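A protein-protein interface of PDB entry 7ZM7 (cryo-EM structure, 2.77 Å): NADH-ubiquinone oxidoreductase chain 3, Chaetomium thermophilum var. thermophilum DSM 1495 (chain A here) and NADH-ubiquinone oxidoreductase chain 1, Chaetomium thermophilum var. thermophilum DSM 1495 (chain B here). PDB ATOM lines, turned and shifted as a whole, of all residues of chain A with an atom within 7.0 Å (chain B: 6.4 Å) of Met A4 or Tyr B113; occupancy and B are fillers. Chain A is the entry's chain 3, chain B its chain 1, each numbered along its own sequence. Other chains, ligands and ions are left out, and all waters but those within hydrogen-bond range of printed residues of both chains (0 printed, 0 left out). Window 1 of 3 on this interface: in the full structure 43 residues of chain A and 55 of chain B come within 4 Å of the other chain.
Ser B9 touches Ser A2.
Val B13 touches Ala A3.
Ala A3 touches Val B104.
Ala B94 touches Met A4 (CB to SD, 3.8 Å).
CE of Met A4 touches OH of Tyr B113, 3.2 Å away.
Ser B9 touches Ile A6.
Tyr A7 touches Val B13.
Tyr B93 touches Tyr A7.
Tyr A7 touches Ala B94.
Ile A8 touches Leu B91.
OG of Ser B9 sits at hydrogen-bond distance from O of Met A1, at 3.0 Å.
Of chain B, only Ala B94 (3.8 Å) and Tyr B113 (3.2 Å) come within 4 Å of Met A4.
Of the printed residues of chain A, Tyr B113 touches Met A4 (3.2 Å).
Of the printed residues of chain A, Val B13 touches Ala A3 (3.8 Å) and Tyr A7 (3.6 Å).
Of the printed residues of chain B, Ala A3 touches Ser B9, Val B13 and Val B104.
Printed residues of chain A within 4 Å of Ser B9: Met A1 (3.0 Å), Ser A2 (3.6 Å), Ala A3 (3.7 Å) and Ile A6 (3.6 Å).
Of the printed residues of chain A, Leu B91 touches Ile A8.
Met B114 touches none of the printed residues of chain A.
Gly B92 touches none of the printed residues of chain A.
The nearest residue of chain B that does not touch Met A4 is Asn B105 (4.1 Å).
The nearest residue of chain A that does not touch Tyr B113 is Ile A8 (5.9 Å).
Hydrophobic or aromatic side chains of chain A within 4 Å of the printed part of chain B: Ala A3, Met A4, Ile A6, Tyr A7 and Ile A8.
Along chain A the printed residues that touch a printed residue of chain B span positions 1 to 8.
Printed residues of chain B that touch a printed residue of chain A: Ser B9, Val B13, Leu B91, Tyr B93, Ala B94, Val B104 and Tyr B113.
Hydrophobic or aromatic side chains of chain B within 4 Å of the printed part of chain A: Val B13, Leu B91, Tyr B93, Ala B94 and Tyr B113.
Among the printed residues, 12 pairs touch across the chains.
Among the printed residues, no Asp or Glu carboxylate lies within 4 Å of a Lys or Arg side-chain nitrogen of the other chain.
The side-chain hydroxyl of Tyr B113 lies within hydrogen-bond range of the backbone carbonyl oxygen of Leu B91 (2.9 Å).
The backbone NH of Asn B105 sits at hydrogen-bond distance from the backbone carbonyl oxygen of Ala B94 (3.0 Å).
O of Ser A2 lies within hydrogen-bond range of OG of Ser A5, 2.9 Å away.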
ATOM      1  N   MET A   1      27.127  -1.160   8.775  1.00  0.00           N
ATOM      2  CA  MET A   1      26.060  -0.675   9.641  1.00  0.00           C
ATOM      3  C   MET A   1      25.331   0.492   8.996  1.00  0.00           C
ATOM      4  O   MET A   1      25.737   0.987   7.948  1.00  0.00           O
ATOM      5  CB  MET A   1      26.617  -0.250  10.998  1.00  0.00           C
ATOM      6  CG  MET A   1      27.177  -1.386  11.827  1.00  0.00           C
ATOM      7  SD  MET A   1      27.758  -0.830  13.438  1.00  0.00           S
ATOM      8  CE  MET A   1      29.270   0.008  12.979  1.00  0.00           C
ATOM      9  N   SER A   2      24.252   0.933   9.636  1.00  0.00           N
ATOM     10  CA  SER A   2      23.510   2.084   9.146  1.00  0.00           C
ATOM     11  C   SER A   2      24.327   3.356   9.323  1.00  0.00           C
ATOM     12  O   SER A   2      25.282   3.406  10.099  1.00  0.00           O
ATOM     13  CB  SER A   2      22.181   2.218   9.884  1.00  0.00           C
ATOM     14  OG  SER A   2      22.382   2.731  11.189  1.00  0.00           O
ATOM     15  N   ALA A   3      23.904   4.428   8.662  1.00  0.00           N
ATOM     16  CA  ALA A   3      24.633   5.708   8.796  1.00  0.00           C
ATOM     17  C   ALA A   3      24.212   6.435  10.075  1.00  0.00           C
ATOM     18  O   ALA A   3      25.083   7.063  10.688  1.00  0.00           O
ATOM     19  CB  ALA A   3      24.406   6.561   7.582  1.00  0.00           C
ATOM     20  N   MET A   4      22.941   6.335  10.475  1.00  0.00           N
ATOM     21  CA  MET A   4      22.474   7.114  11.655  1.00  0.00           C
ATOM     22  C   MET A   4      23.223   6.630  12.890  1.00  0.00           C
ATOM     23  O   MET A   4      23.656   7.469  13.689  1.00  0.00           O
ATOM     24  CB  MET A   4      20.971   6.930  11.885  1.00  0.00           C
ATOM     25  CG  MET A   4      20.348   8.021  12.716  1.00  0.00           C
ATOM     26  SD  MET A   4      20.785   9.652  12.083  1.00  0.00           S
ATOM     27  CE  MET A   4      19.531  10.644  12.885  1.00  0.00           C
ATOM     28  N   SER A   5      23.473   5.328  12.982  1.00  0.00           N
ATOM     29  CA  SER A   5      24.211   4.784  14.148  1.00  0.00           C
ATOM     30  C   SER A   5      25.638   5.344  14.190  1.00  0.00           C
ATOM     31  O   SER A   5      25.999   5.910  15.231  1.00  0.00           O
ATOM     32  CB  SER A   5      24.218   3.285  14.097  1.00  0.00           C
ATOM     33  OG  SER A   5      24.730   2.824  12.855  1.00  0.00           O
ATOM     34  N   ILE A   6      26.397   5.248  13.097  1.00  0.00           N
ATOM     35  CA  ILE A   6      27.823   5.702  13.093  1.00  0.00           C
ATOM     36  C   ILE A   6      27.869   7.197  13.418  1.00  0.00           C
ATOM     37  O   ILE A   6      28.765   7.594  14.159  1.00  0.00           O
ATOM     38  CB  ILE A   6      28.553   5.302  11.794  1.00  0.00           C
ATOM     39  CG1 ILE A   6      28.589   3.782  11.638  1.00  0.00           C
ATOM     40  CG2 ILE A   6      29.944   5.905  11.733  1.00  0.00           C
ATOM     41  CD1 ILE A   6      29.602   3.290  10.640  1.00  0.00           C
ATOM     42  N   TYR A   7      26.894   7.968  12.940  1.00  0.00           N
ATOM     43  CA  TYR A   7      26.811   9.421  13.236  1.00  0.00           C
ATOM     44  C   TYR A   7      26.670   9.711  14.739  1.00  0.00           C
ATOM     45  O   TYR A   7      27.367  10.609  15.216  1.00  0.00           O
ATOM     46  CB  TYR A   7      25.616  10.020  12.486  1.00  0.00           C
ATOM     47  CG  TYR A   7      25.513  11.517  12.609  1.00  0.00           C
ATOM     48  CD1 TYR A   7      26.202  12.344  11.744  1.00  0.00           C
ATOM     49  CD2 TYR A   7      24.751  12.105  13.607  1.00  0.00           C
ATOM     50  CE1 TYR A   7      26.131  13.720  11.857  1.00  0.00           C
ATOM     51  CE2 TYR A   7      24.675  13.480  13.738  1.00  0.00           C
ATOM     52  CZ  TYR A   7      25.366  14.287  12.857  1.00  0.00           C
ATOM     53  OH  TYR A   7      25.303  15.640  12.961  1.00  0.00           O
ATOM     54  N   ILE A   8      25.795   9.025  15.468  1.00  0.00           N
ATOM     55  CA  ILE A   8      25.652   9.379  16.912  1.00  0.00           C
ATOM     56  C   ILE A   8      26.938   9.001  17.637  1.00  0.00           C
ATOM     57  O   ILE A   8      27.434   9.830  18.413  1.00  0.00           O
ATOM     58  CB  ILE A   8      24.417   8.736  17.564  1.00  0.00           C
ATOM     59  CG1 ILE A   8      23.168   8.933  16.700  1.00  0.00           C
ATOM     60  CG2 ILE A   8      24.213   9.254  18.976  1.00  0.00           C
ATOM     61  CD1 ILE A   8      21.932   8.257  17.243  1.00  0.00           C
ATOM     62  N   ILE A   9      27.489   7.829  17.322  1.00  0.00           N
ATOM     63  CA  ILE A   9      28.719   7.356  18.016  1.00  0.00           C
ATOM     64  C   ILE A   9      29.834   8.371  17.752  1.00  0.00           C
ATOM     65  O   ILE A   9      30.580   8.664  18.683  1.00  0.00           O
ATOM     66  CB  ILE A   9      29.106   5.945  17.535  1.00  0.00           C
ATOM     67  CG1 ILE A   9      27.956   4.951  17.710  1.00  0.00           C
ATOM     68  CG2 ILE A   9      30.371   5.460  18.224  1.00  0.00           C
ATOM     69  CD1 ILE A   9      28.188   3.622  17.032  1.00  0.00           C
ATOM     70  N   SER B   9      29.068   4.678   5.395  1.00  0.00           N
ATOM     71  CA  SER B   9      28.506   5.362   6.584  1.00  0.00           C
ATOM     72  C   SER B   9      29.551   6.330   7.145  1.00  0.00           C
ATOM     73  O   SER B   9      29.211   7.507   7.318  1.00  0.00           O
ATOM     74  CB  SER B   9      28.066   4.356   7.605  1.00  0.00           C
ATOM     75  OG  SER B   9      27.124   3.453   7.052  1.00  0.00           O
ATOM     76  N   VAL B  13      29.341  10.688   7.290  1.00  0.00           N
ATOM     77  CA  VAL B  13      29.290  11.298   8.649  1.00  0.00           C
ATOM     78  C   VAL B  13      30.478  12.246   8.867  1.00  0.00           C
ATOM     79  O   VAL B  13      30.239  13.349   9.381  1.00  0.00           O
ATOM     80  CB  VAL B  13      29.207  10.201   9.728  1.00  0.00           C
ATOM     81  CG1 VAL B  13      29.510  10.719  11.122  1.00  0.00           C
ATOM     82  CG2 VAL B  13      27.880   9.464   9.684  1.00  0.00           C
ATOM     83  N   LEU B  91      22.731  16.555  16.648  1.00  0.00           N
ATOM     84  CA  LEU B  91      21.881  15.433  16.147  1.00  0.00           C
ATOM     85  C   LEU B  91      20.902  15.906  15.072  1.00  0.00           C
ATOM     86  O   LEU B  91      20.314  15.043  14.406  1.00  0.00           O
ATOM     87  CB  LEU B  91      21.109  14.802  17.312  1.00  0.00           C
ATOM     88  CG  LEU B  91      21.727  13.543  17.910  1.00  0.00           C
ATOM     89  CD1 LEU B  91      20.806  12.939  18.957  1.00  0.00           C
ATOM     90  CD2 LEU B  91      22.034  12.525  16.823  1.00  0.00           C
ATOM     91  N   GLY B  92      20.717  17.243  14.949  1.00  0.00           N
ATOM     92  CA  GLY B  92      19.763  17.749  13.946  1.00  0.00           C
ATOM     93  C   GLY B  92      20.353  17.809  12.556  1.00  0.00           C
ATOM     94  O   GLY B  92      19.575  17.890  11.597  1.00  0.00           O
ATOM     95  N   TYR B  93      21.680  17.797  12.452  1.00  0.00           N
ATOM     96  CA  TYR B  93      22.378  17.952  11.153  1.00  0.00           C
ATOM     97  C   TYR B  93      22.272  16.675  10.329  1.00  0.00           C
ATOM     98  O   TYR B  93      22.568  16.734   9.138  1.00  0.00           O
ATOM     99  CB  TYR B  93      23.837  18.362  11.372  1.00  0.00           C
ATOM    100  CG  TYR B  93      24.062  19.799  11.757  1.00  0.00           C
ATOM    101  CD1 TYR B  93      23.859  20.234  13.057  1.00  0.00           C
ATOM    102  CD2 TYR B  93      24.505  20.722  10.825  1.00  0.00           C
ATOM    103  CE1 TYR B  93      24.074  21.554  13.417  1.00  0.00           C
ATOM    104  CE2 TYR B  93      24.723  22.045  11.169  1.00  0.00           C
ATOM    105  CZ  TYR B  93      24.507  22.462  12.468  1.00  0.00           C
ATOM    106  OH  TYR B  93      24.720  23.761  12.817  1.00  0.00           O
ATOM    107  N   ALA B  94      21.830  15.579  10.932  1.00  0.00           N
ATOM    108  CA  ALA B  94      21.796  14.266  10.249  1.00  0.00           C
ATOM    109  C   ALA B  94      20.601  14.146   9.298  1.00  0.00           C
ATOM    110  O   ALA B  94      20.488  13.099   8.647  1.00  0.00           O
ATOM    111  CB  ALA B  94      21.818  13.178  11.282  1.00  0.00           C
ATOM    112  N   VAL B  95      19.755  15.171   9.192  1.00  0.00           N
ATOM    113  CA  VAL B  95      18.670  15.164   8.222  1.00  0.00           C
ATOM    114  C   VAL B  95      18.770  16.307   7.225  1.00  0.00           C
ATOM    115  O   VAL B  95      17.846  16.507   6.437  1.00  0.00           O
ATOM    116  CB  VAL B  95      17.300  15.168   8.908  1.00  0.00           C
ATOM    117  CG1 VAL B  95      17.124  13.914   9.691  1.00  0.00           C
ATOM    118  CG2 VAL B  95      17.178  16.371   9.785  1.00  0.00           C
ATOM    119  N   VAL B 104      22.646  12.357   5.510  1.00  0.00           N
ATOM    120  CA  VAL B 104      23.106  11.164   6.281  1.00  0.00           C
ATOM    121  C   VAL B 104      21.913  10.216   6.362  1.00  0.00           C
ATOM    122  O   VAL B 104      22.042   9.068   5.917  1.00  0.00           O
ATOM    123  CB  VAL B 104      23.614  11.540   7.687  1.00  0.00           C
ATOM    124  CG1 VAL B 104      23.655  10.352   8.634  1.00  0.00           C
ATOM    125  CG2 VAL B 104      24.967  12.228   7.636  1.00  0.00           C
ATOM    126  N   ASN B 105      20.798  10.689   6.912  1.00  0.00           N
ATOM    127  CA  ASN B 105      19.554   9.889   6.954  1.00  0.00           C
ATOM    128  C   ASN B 105      18.511  10.567   6.066  1.00  0.00           C
ATOM    129  O   ASN B 105      18.147  11.708   6.364  1.00  0.00           O
ATOM    130  CB  ASN B 105      19.011   9.810   8.377  1.00  0.00           C
ATOM    131  CG  ASN B 105      17.787   8.933   8.543  1.00  0.00           C
ATOM    132  OD1 ASN B 105      17.343   8.274   7.606  1.00  0.00           O
ATOM    133  ND2 ASN B 105      17.242   8.909   9.746  1.00  0.00           N
ATOM    134  N   LEU B 107      15.038  10.831   5.675  1.00  0.00           N
ATOM    135  CA  LEU B 107      13.902  10.394   6.529  1.00  0.00           C
ATOM    136  C   LEU B 107      12.587  10.990   6.043  1.00  0.00           C
ATOM    137  O   LEU B 107      12.555  12.199   5.793  1.00  0.00           O
ATOM    138  CB  LEU B 107      14.213  10.813   7.971  1.00  0.00           C
ATOM    139  CG  LEU B 107      13.363  10.147   9.048  1.00  0.00           C
ATOM    140  CD1 LEU B 107      13.628   8.650   9.092  1.00  0.00           C
ATOM    141  CD2 LEU B 107      13.621  10.777  10.406  1.00  0.00           C
ATOM    142  N   THR B 109       9.863  11.153   7.760  1.00  0.00           N
ATOM    143  CA  THR B 109       9.428  12.009   8.880  1.00  0.00           C
ATOM    144  C   THR B 109      10.586  12.915   9.301  1.00  0.00           C
ATOM    145  O   THR B 109      10.748  13.110  10.510  1.00  0.00           O
ATOM    146  CB  THR B 109       8.935  11.143  10.047  1.00  0.00           C
ATOM    147  OG1 THR B 109       9.939  10.162  10.305  1.00  0.00           O
ATOM    148  CG2 THR B 109       7.616  10.461   9.763  1.00  0.00           C
ATOM    149  N   GLY B 110      11.357  13.441   8.348  1.00  0.00           N
ATOM    150  CA  GLY B 110      12.505  14.266   8.685  1.00  0.00           C
ATOM    151  C   GLY B 110      12.145  15.495   9.494  1.00  0.00           C
ATOM    152  O   GLY B 110      12.896  15.905  10.377  1.00  0.00           O
ATOM    153  N   ILE B 111      10.999  16.101   9.202  1.00  0.00           N
ATOM    154  CA  ILE B 111      10.554  17.273   9.943  1.00  0.00           C
ATOM    155  C   ILE B 111      10.221  16.903  11.384  1.00  0.00           C
ATOM    156  O   ILE B 111      10.580  17.612  12.328  1.00  0.00           O
ATOM    157  CB  ILE B 111       9.355  17.924   9.230  1.00  0.00           C
ATOM    158  CG1 ILE B 111       9.804  18.622   7.950  1.00  0.00           C
ATOM    159  CG2 ILE B 111       8.664  18.892  10.137  1.00  0.00           C
ATOM    160  CD1 ILE B 111      10.932  19.601   8.127  1.00  0.00           C
ATOM    161  N   LEU B 112       9.559  15.762  11.599  1.00  0.00           N
ATOM    162  CA  LEU B 112       9.134  15.429  12.983  1.00  0.00           C
ATOM    163  C   LEU B 112      10.371  15.000  13.768  1.00  0.00           C
ATOM    164  O   LEU B 112      10.303  14.999  15.006  1.00  0.00           O
ATOM    165  CB  LEU B 112       8.063  14.338  12.947  1.00  0.00           C
ATOM    166  CG  LEU B 112       6.661  14.822  12.592  1.00  0.00           C
ATOM    167  CD1 LEU B 112       5.724  13.642  12.420  1.00  0.00           C
ATOM    168  CD2 LEU B 112       6.135  15.771  13.655  1.00  0.00           C
ATOM    169  N   TYR B 113      11.453  14.660  13.069  1.00  0.00           N
ATOM    170  CA  TYR B 113      12.743  14.353  13.734  1.00  0.00           C
ATOM    171  C   TYR B 113      13.325  15.627  14.334  1.00  0.00           C
ATOM    172  O   TYR B 113      13.887  15.568  15.433  1.00  0.00           O
ATOM    173  CB  TYR B 113      13.745  13.764  12.740  1.00  0.00           C
ATOM    174  CG  TYR B 113      15.085  13.491  13.366  1.00  0.00           C
ATOM    175  CD1 TYR B 113      15.222  12.519  14.342  1.00  0.00           C
ATOM    176  CD2 TYR B 113      16.201  14.233  13.023  1.00  0.00           C
ATOM    177  CE1 TYR B 113      16.442  12.273  14.946  1.00  0.00           C
ATOM    178  CE2 TYR B 113      17.430  13.994  13.609  1.00  0.00           C
ATOM    179  CZ  TYR B 113      17.548  13.014  14.576  1.00  0.00           C
ATOM    180  OH  TYR B 113      18.751  12.765  15.161  1.00  0.00           O
ATOM    181  N   MET B 114      13.265  16.732  13.582  1.00  0.00           N
ATOM    182  CA  MET B 114      13.894  18.013  14.010  1.00  0.00           C
ATOM    183  C   MET B 114      12.983  18.746  14.987  1.00  0.00           C
ATOM    184  O   MET B 114      13.408  19.773  15.523  1.00  0.00           O
ATOM    185  CB  MET B 114      14.176  18.916  12.813  1.00  0.00           C
ATOM    186  CG  MET B 114      15.522  18.660  12.179  1.00  0.00           C
ATOM    187  SD  MET B 114      15.575  19.533  10.609  1.00  0.00           S
ATOM    188  CE  MET B 114      13.861  19.341  10.131  1.00  0.00           C
ATOM    189  N   LEU B 115      11.798  18.202  15.229  1.00  0.00           N
ATOM    190  CA  LEU B 115      10.849  18.803  16.191  1.00  0.00           C
ATOM    191  C   LEU B 115      11.094  18.072  17.501  1.00  0.00           C
ATOM    192  O   LEU B 115      10.883  18.676  18.562  1.00  0.00           O
ATOM    193  CB  LEU B 115       9.417  18.609  15.686  1.00  0.00           C
ATOM    194  CG  LEU B 115       8.937  19.632  14.659  1.00  0.00           C
ATOM    195  CD1 LEU B 115       7.487  19.377  14.285  1.00  0.00           C
ATOM    196  CD2 LEU B 115       9.106  21.047  15.186  1.00  0.00           C
ATOM    197  N   ALA B 116      11.532  16.811  17.405  1.00  0.00           N
ATOM    198  CA  ALA B 116      11.882  16.069  18.612  1.00  0.00           C
ATOM    199  C   ALA B 116      13.183  16.568  19.220  1.00  0.00           C
ATOM    200  O   ALA B 116      13.258  16.780  20.432  1.00  0.00           O
ATOM    201  CB  ALA B 116      11.980  14.577  18.318  1.00  0.00           C
ATOM    202  N   VAL B 117      14.208  16.711  18.379  1.00  0.00           N
ATOM    203  CA  VAL B 117      15.552  17.154  18.856  1.00  0.00           C
ATOM    204  C   VAL B 117      15.465  18.585  19.391  1.00  0.00           C
ATOM    205  O   VAL B 117      16.367  18.977  20.153  1.00  0.00           O
ATOM    206  CB  VAL B 117      16.653  16.990  17.790  1.00  0.00           C
ATOM    207  CG1 VAL B 117      16.831  15.540  17.371  1.00  0.00           C
ATOM    208  CG2 VAL B 117      16.439  17.887  16.582  1.00  0.00           C
ATOM    209  N   SER B 118      14.424  19.327  19.017  1.00  0.00           N
ATOM    210  CA  SER B 118      14.338  20.750  19.425  1.00  0.00           C
ATOM    211  C   SER B 118      13.706  20.831  20.806  1.00  0.00           C
ATOM    212  O   SER B 118      14.087  21.717  21.576  1.00  0.00           O
ATOM    213  CB  SER B 118      13.529  21.530  18.438  1.00  0.00           C
ATOM    214  OG  SER B 118      13.483  22.901  18.804  1.00  0.00           O
